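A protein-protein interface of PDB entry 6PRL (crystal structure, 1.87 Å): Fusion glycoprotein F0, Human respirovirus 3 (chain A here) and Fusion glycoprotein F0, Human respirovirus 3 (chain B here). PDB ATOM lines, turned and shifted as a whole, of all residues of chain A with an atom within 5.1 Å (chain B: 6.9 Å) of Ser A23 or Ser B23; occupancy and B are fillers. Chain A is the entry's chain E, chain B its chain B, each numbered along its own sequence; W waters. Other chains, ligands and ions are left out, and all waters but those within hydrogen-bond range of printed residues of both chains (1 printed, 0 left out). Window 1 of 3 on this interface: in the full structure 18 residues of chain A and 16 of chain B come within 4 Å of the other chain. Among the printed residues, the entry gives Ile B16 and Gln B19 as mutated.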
ATOM      1  N   LYS A  19      -7.741  22.481 -17.263  1.00  0.00           N
ATOM      2  CA  LYS A  19      -6.450  22.326 -16.598  1.00  0.00           C
ATOM      3  C   LYS A  19      -6.546  22.685 -15.116  1.00  0.00           C
ATOM      4  O   LYS A  19      -5.893  22.057 -14.274  1.00  0.00           O
ATOM      5  CB  LYS A  19      -5.392  23.165 -17.312  1.00  0.00           C
ATOM      6  CG  LYS A  19      -4.864  22.500 -18.583  1.00  0.00           C
ATOM      7  CD  LYS A  19      -3.905  23.386 -19.357  1.00  0.00           C
ATOM      8  CE  LYS A  19      -4.631  24.545 -20.021  1.00  0.00           C
ATOM      9  NZ  LYS A  19      -3.793  25.218 -21.054  1.00  0.00           N
ATOM     10  N   ALA A  20      -7.364  23.684 -14.772  1.00  0.00           N
ATOM     11  CA  ALA A  20      -7.586  23.999 -13.363  1.00  0.00           C
ATOM     12  C   ALA A  20      -8.225  22.820 -12.637  1.00  0.00           C
ATOM     13  O   ALA A  20      -7.884  22.529 -11.485  1.00  0.00           O
ATOM     14  CB  ALA A  20      -8.461  25.246 -13.233  1.00  0.00           C
ATOM     15  N   VAL A  21      -9.154  22.128 -13.300  1.00  0.00           N
ATOM     16  CA  VAL A  21      -9.797  20.970 -12.690  1.00  0.00           C
ATOM     17  C   VAL A  21      -8.803  19.825 -12.545  1.00  0.00           C
ATOM     18  O   VAL A  21      -8.822  19.091 -11.550  1.00  0.00           O
ATOM     19  CB  VAL A  21     -11.031  20.553 -13.511  1.00  0.00           C
ATOM     20  CG1 VAL A  21     -11.598  19.238 -12.990  1.00  0.00           C
ATOM     21  CG2 VAL A  21     -12.082  21.645 -13.468  1.00  0.00           C
ATOM     22  N   GLN A  22      -7.915  19.650 -13.529  1.00  0.00           N
ATOM     23  CA  GLN A  22      -6.917  18.591 -13.432  1.00  0.00           C
ATOM     24  C   GLN A  22      -5.975  18.829 -12.258  1.00  0.00           C
ATOM     25  O   GLN A  22      -5.597  17.883 -11.551  1.00  0.00           O
ATOM     26  CB  GLN A  22      -6.139  18.484 -14.743  1.00  0.00           C
ATOM     27  CG  GLN A  22      -6.939  17.858 -15.864  1.00  0.00           C
ATOM     28  CD  GLN A  22      -6.139  17.726 -17.145  1.00  0.00           C
ATOM     29  OE1 GLN A  22      -5.299  18.570 -17.457  1.00  0.00           O
ATOM     30  NE2 GLN A  22      -6.395  16.659 -17.891  1.00  0.00           N
ATOM     31  N   SER A  23      -5.582  20.085 -12.029  1.00  0.00           N
ATOM     32  CA  SER A  23      -4.771  20.394 -10.857  1.00  0.00           C
ATOM     33  C   SER A  23      -5.520  20.060  -9.575  1.00  0.00           C
ATOM     34  O   SER A  23      -4.935  19.516  -8.629  1.00  0.00           O
ATOM     35  CB  SER A  23      -4.362  21.865 -10.868  1.00  0.00           C
ATOM     36  OG  SER A  23      -3.434  22.133 -11.904  1.00  0.00           O
ATOM     37  N   VAL A  24      -6.812  20.389  -9.517  1.00  0.00           N
ATOM     38  CA  VAL A  24      -7.625  20.028  -8.358  1.00  0.00           C
ATOM     39  C   VAL A  24      -7.670  18.514  -8.192  1.00  0.00           C
ATOM     40  O   VAL A  24      -7.620  17.994  -7.069  1.00  0.00           O
ATOM     41  CB  VAL A  24      -9.040  20.621  -8.495  1.00  0.00           C
ATOM     42  CG1 VAL A  24     -10.014  19.912  -7.556  1.00  0.00           C
ATOM     43  CG2 VAL A  24      -9.019  22.111  -8.202  1.00  0.00           C
ATOM     44  N   GLN A  25      -7.778  17.783  -9.305  1.00  0.00           N
ATOM     45  CA  GLN A  25      -7.792  16.327  -9.234  1.00  0.00           C
ATOM     46  C   GLN A  25      -6.504  15.796  -8.621  1.00  0.00           C
ATOM     47  O   GLN A  25      -6.533  14.863  -7.810  1.00  0.00           O
ATOM     48  CB  GLN A  25      -8.007  15.743 -10.630  1.00  0.00           C
ATOM     49  CG  GLN A  25      -9.424  15.932 -11.142  1.00  0.00           C
ATOM     50  CD  GLN A  25      -9.556  15.682 -12.631  1.00  0.00           C
ATOM     51  OE1 GLN A  25      -8.563  15.499 -13.335  1.00  0.00           O
ATOM     52  NE2 GLN A  25     -10.788  15.682 -13.115  1.00  0.00           N
ATOM     53  N   SER A  26      -5.363  16.384  -8.990  1.00  0.00           N
ATOM     54  CA  SER A  26      -4.095  15.973  -8.395  1.00  0.00           C
ATOM     55  C   SER A  26      -4.061  16.294  -6.905  1.00  0.00           C
ATOM     56  O   SER A  26      -3.566  15.495  -6.099  1.00  0.00           O
ATOM     57  CB  SER A  26      -2.936  16.653  -9.121  1.00  0.00           C
ATOM     58  OG  SER A  26      -2.942  16.331 -10.501  1.00  0.00           O
ATOM     59  N   SER A  27      -4.597  17.453  -6.515  1.00  0.00           N
ATOM     60  CA  SER A  27      -4.578  17.828  -5.105  1.00  0.00           C
ATOM     61  C   SER A  27      -5.392  16.850  -4.265  1.00  0.00           C
ATOM     62  O   SER A  27      -5.011  16.528  -3.131  1.00  0.00           O
ATOM     63  CB  SER A  27      -5.105  19.252  -4.936  1.00  0.00           C
ATOM     64  OG  SER A  27      -6.494  19.321  -5.207  1.00  0.00           O
ATOM     65  N   ILE B  16       0.084  19.798  -2.151  1.00  0.00           N
ATOM     66  CA  ILE B  16      -1.318  20.156  -2.355  1.00  0.00           C
ATOM     67  C   ILE B  16      -1.464  21.663  -2.519  1.00  0.00           C
ATOM     68  O   ILE B  16      -2.147  22.145  -3.431  1.00  0.00           O
ATOM     69  CB  ILE B  16      -2.183  19.635  -1.192  1.00  0.00           C
ATOM     70  CG1 ILE B  16      -2.172  18.108  -1.156  1.00  0.00           C
ATOM     71  CG2 ILE B  16      -3.606  20.161  -1.332  1.00  0.00           C
ATOM     72  CD1 ILE B  16      -2.686  17.528   0.145  1.00  0.00           C
ATOM     73  N   SER B  18       0.765  23.747  -3.522  1.00  0.00           N
ATOM     74  CA  SER B  18       1.369  24.148  -4.790  1.00  0.00           C
ATOM     75  C   SER B  18       0.436  23.858  -5.961  1.00  0.00           C
ATOM     76  O   SER B  18       0.343  24.655  -6.907  1.00  0.00           O
ATOM     77  CB  SER B  18       2.706  23.432  -4.979  1.00  0.00           C
ATOM     78  OG  SER B  18       3.283  23.750  -6.231  1.00  0.00           O
ATOM     79  N   GLN B  19      -0.261  22.721  -5.919  1.00  0.00           N
ATOM     80  CA  GLN B  19      -1.180  22.373  -6.998  1.00  0.00           C
ATOM     81  C   GLN B  19      -2.418  23.262  -6.988  1.00  0.00           C
ATOM     82  O   GLN B  19      -2.986  23.543  -8.055  1.00  0.00           O
ATOM     83  CB  GLN B  19      -1.566  20.897  -6.890  1.00  0.00           C
ATOM     84  CG  GLN B  19      -0.409  19.945  -7.190  1.00  0.00           C
ATOM     85  CD  GLN B  19      -0.713  18.505  -6.834  1.00  0.00           C
ATOM     86  OE1 GLN B  19      -1.456  18.225  -5.890  1.00  0.00           O
ATOM     87  NE2 GLN B  19      -0.127  17.577  -7.584  1.00  0.00           N
ATOM     88  N   LEU B  20      -2.855  23.710  -5.808  1.00  0.00           N
ATOM     89  CA  LEU B  20      -3.976  24.641  -5.744  1.00  0.00           C
ATOM     90  C   LEU B  20      -3.604  25.986  -6.351  1.00  0.00           C
ATOM     91  O   LEU B  20      -4.423  26.614  -7.034  1.00  0.00           O
ATOM     92  CB  LEU B  20      -4.436  24.822  -4.297  1.00  0.00           C
ATOM     93  CG  LEU B  20      -5.265  23.692  -3.694  1.00  0.00           C
ATOM     94  CD1 LEU B  20      -5.461  23.934  -2.202  1.00  0.00           C
ATOM     95  CD2 LEU B  20      -6.607  23.564  -4.394  1.00  0.00           C
ATOM     96  N   GLU B  21      -2.373  26.448  -6.116  1.00  0.00           N
ATOM     97  CA  GLU B  21      -1.932  27.699  -6.722  1.00  0.00           C
ATOM     98  C   GLU B  21      -1.909  27.587  -8.242  1.00  0.00           C
ATOM     99  O   GLU B  21      -2.307  28.520  -8.947  1.00  0.00           O
ATOM    100  CB  GLU B  21      -0.553  28.089  -6.195  1.00  0.00           C
ATOM    101  CG  GLU B  21      -0.556  28.646  -4.778  1.00  0.00           C
ATOM    102  CD  GLU B  21      -1.449  29.864  -4.628  1.00  0.00           C
ATOM    103  OE1 GLU B  21      -2.450  29.778  -3.886  1.00  0.00           O
ATOM    104  OE2 GLU B  21      -1.158  30.900  -5.262  1.00  0.00           O
ATOM    105  N   GLU B  22      -1.446  26.450  -8.767  1.00  0.00           N
ATOM    106  CA  GLU B  22      -1.489  26.240 -10.211  1.00  0.00           C
ATOM    107  C   GLU B  22      -2.926  26.227 -10.716  1.00  0.00           C
ATOM    108  O   GLU B  22      -3.225  26.778 -11.784  1.00  0.00           O
ATOM    109  CB  GLU B  22      -0.780  24.935 -10.571  1.00  0.00           C
ATOM    110  CG  GLU B  22       0.728  24.985 -10.389  1.00  0.00           C
ATOM    111  CD  GLU B  22       1.398  23.658 -10.686  1.00  0.00           C
ATOM    112  OE1 GLU B  22       2.506  23.419 -10.157  1.00  0.00           O
ATOM    113  OE2 GLU B  22       0.818  22.853 -11.445  1.00  0.00           O
ATOM    114  N   SER B  23      -3.834  25.603  -9.963  1.00  0.00           N
ATOM    115  CA  SER B  23      -5.242  25.607 -10.340  1.00  0.00           C
ATOM    116  C   SER B  23      -5.794  27.024 -10.369  1.00  0.00           C
ATOM    117  O   SER B  23      -6.507  27.407 -11.308  1.00  0.00           O
ATOM    118  CB  SER B  23      -6.043  24.735  -9.369  1.00  0.00           C
ATOM    119  OG  SER B  23      -7.409  24.653  -9.752  1.00  0.00           O
ATOM    120  N   LYS B  24      -5.474  27.825  -9.350  1.00  0.00           N
ATOM    121  CA  LYS B  24      -5.975  29.193  -9.306  1.00  0.00           C
ATOM    122  C   LYS B  24      -5.494  29.994 -10.510  1.00  0.00           C
ATOM    123  O   LYS B  24      -6.231  30.831 -11.044  1.00  0.00           O
ATOM    124  CB  LYS B  24      -5.539  29.868  -8.006  1.00  0.00           C
ATOM    125  CG  LYS B  24      -6.272  29.374  -6.766  1.00  0.00           C
ATOM    126  CD  LYS B  24      -5.678  29.966  -5.489  1.00  0.00           C
ATOM    127  CE  LYS B  24      -5.948  31.462  -5.371  1.00  0.00           C
ATOM    128  NZ  LYS B  24      -5.086  32.105  -4.337  1.00  0.00           N
ATOM    129  N   GLU B  25      -4.263  29.749 -10.956  1.00  0.00           N
ATOM    130  CA  GLU B  25      -3.727  30.519 -12.072  1.00  0.00           C
ATOM    131  C   GLU B  25      -4.349  30.094 -13.398  1.00  0.00           C
ATOM    132  O   GLU B  25      -4.518  30.931 -14.291  1.00  0.00           O
ATOM    133  CB  GLU B  25      -2.207  30.384 -12.122  1.00  0.00           C
ATOM    134  CG  GLU B  25      -1.475  31.171 -11.041  1.00  0.00           C
ATOM    135  CD  GLU B  25      -1.895  32.632 -10.989  1.00  0.00           C
ATOM    136  OE1 GLU B  25      -2.670  32.998 -10.079  1.00  0.00           O
ATOM    137  OE2 GLU B  25      -1.467  33.407 -11.871  1.00  0.00           O
ATOM    138  N   TRP B  26      -4.697  28.814 -13.553  1.00  0.00           N
ATOM    139  CA  TRP B  26      -5.384  28.393 -14.767  1.00  0.00           C
ATOM    140  C   TRP B  26      -6.757  29.048 -14.871  1.00  0.00           C
ATOM    141  O   TRP B  26      -7.198  29.416 -15.968  1.00  0.00           O
ATOM    142  CB  TRP B  26      -5.512  26.871 -14.821  1.00  0.00           C
ATOM    143  CG  TRP B  26      -4.252  26.176 -15.221  1.00  0.00           C
ATOM    144  CD1 TRP B  26      -3.549  25.261 -14.487  1.00  0.00           C
ATOM    145  CD2 TRP B  26      -3.534  26.335 -16.453  1.00  0.00           C
ATOM    146  NE1 TRP B  26      -2.442  24.841 -15.187  1.00  0.00           N
ATOM    147  CE2 TRP B  26      -2.410  25.485 -16.396  1.00  0.00           C
ATOM    148  CE3 TRP B  26      -3.732  27.112 -17.599  1.00  0.00           C
ATOM    149  CZ2 TRP B  26      -1.489  25.395 -17.436  1.00  0.00           C
ATOM    150  CZ3 TRP B  26      -2.818  27.018 -18.632  1.00  0.00           C
ATOM    151  CH2 TRP B  26      -1.710  26.166 -18.544  1.00  0.00           C
ATOM    152  N   ILE B  27      -7.451  29.208 -13.739  1.00  0.00           N
ATOM    153  CA  ILE B  27      -8.714  29.941 -13.748  1.00  0.00           C
ATOM    154  C   ILE B  27      -8.470  31.406 -14.092  1.00  0.00           C
ATOM    155  O   ILE B  27      -9.251  32.025 -14.825  1.00  0.00           O
ATOM    156  CB  ILE B  27      -9.433  29.791 -12.395  1.00  0.00           C
ATOM    157  CG1 ILE B  27      -9.967  28.363 -12.232  1.00  0.00           C
ATOM    158  CG2 ILE B  27     -10.557  30.814 -12.270  1.00  0.00           C
ATOM    159  CD1 ILE B  27     -10.989  27.940 -13.268  1.00  0.00           C
ATOM    160  N   ARG B  28      -7.390  31.987 -13.566  1.00  0.00           N
ATOM    161  CA  ARG B  28      -7.054  33.363 -13.913  1.00  0.00           C
ATOM    162  C   ARG B  28      -6.840  33.505 -15.415  1.00  0.00           C
ATOM    163  O   ARG B  28      -7.346  34.449 -16.037  1.00  0.00           O
ATOM    164  CB  ARG B  28      -5.809  33.807 -13.146  1.00  0.00           C
ATOM    165  CG  ARG B  28      -5.603  35.311 -13.122  1.00  0.00           C
ATOM    166  CD  ARG B  28      -4.168  35.677 -12.780  1.00  0.00           C
ATOM    167  NE  ARG B  28      -3.232  35.191 -13.791  1.00  0.00           N
ATOM    168  CZ  ARG B  28      -3.018  35.782 -14.963  1.00  0.00           C
ATOM    169  NH1 ARG B  28      -3.676  36.888 -15.285  1.00  0.00           N
ATOM    170  NH2 ARG B  28      -2.147  35.263 -15.816  1.00  0.00           N
HETATM  171  O   HOH W   1      -1.150  21.427 -10.656  1.00  0.00           O
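The backbone carbonyl oxygen (O) of Ala A20 sits at hydrogen-bond distance from the side-chain hydroxyl (OG) of Ser B23, 2.8 Å away. O of Ser A26 sits close to OE1 of Gln B19 (3.5 Å). The backbone NH of Ser A27 lies close to the side-chain amide oxygen of Gln B19.
The side-chain hydroxyl of Ser A23 lies within hydrogen-bond range of the backbone carbonyl oxygen of Lys A19. OG of Ser A26 sits at hydrogen-bond distance from O of Gln A22. O of Val A24 lies within hydrogen-bond range of OG of Ser A27, 2.5 Å away.
Among the printed residues, pairs that only touch across the chains: Lys A19 with Trp B26, Val A24 with Ser B23, Ser A23 with Gln B19, Ala A20 with Ile B27, Ser A23 with Ser B23, Ala A20 with Trp B26 and Ser A27 with Ile B16.
Of the printed residues of chain B, Ala A20 touches Ser B23 (2.8 Å), Trp B26 (3.7 Å) and Ile B27 (3.6 Å). Ser A23 touches just these residues of chain B: Gln B19 (3.6 Å) and Ser B23 (3.6 Å). Printed residues of chain A within 4 Å of Ile B16: Ser A27. Printed residues of chain A within 4 Å of Gln B19: Ser A23 (3.6 Å), Ser A26 (3.3 Å) and Ser A27 (3.2 Å). Of the printed residues of chain A, Ser B23 touches Ala A20 (2.8 Å), Ser A23 (3.6 Å) and Val A24 (3.4 Å). Of the printed residues of chain A, Ile B27 touches Ala A20 (3.6 Å). The nearest printed residue of chain B that does not touch Ser A23 is Trp B26 (4.1 Å). The nearest printed residue of chain B that does not touch Lys A19 is Ser B23 (5.3 Å).
Printed residues of chain B that touch a printed residue of chain A: Ile B16, Gln B19, Ser B23, Trp B26 and Ile B27. Hydrophobic or aromatic side chains of chain B within 4 Å of the printed part of chain A: Ile B16, Trp B26 and Ile B27. Of the 9 printed residues of chain A, 6 touch a printed residue of chain B. Among the printed residues, no Asp or Glu carboxylate lies within 4 Å of a Lys or Arg side-chain nitrogen of the other chain.
Water W1 lies within hydrogen-bond range of the side-chain carboxylate of Glu B22 (2.6 Å) and the side-chain hydroxyl of Ser A23 (2.7 Å).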
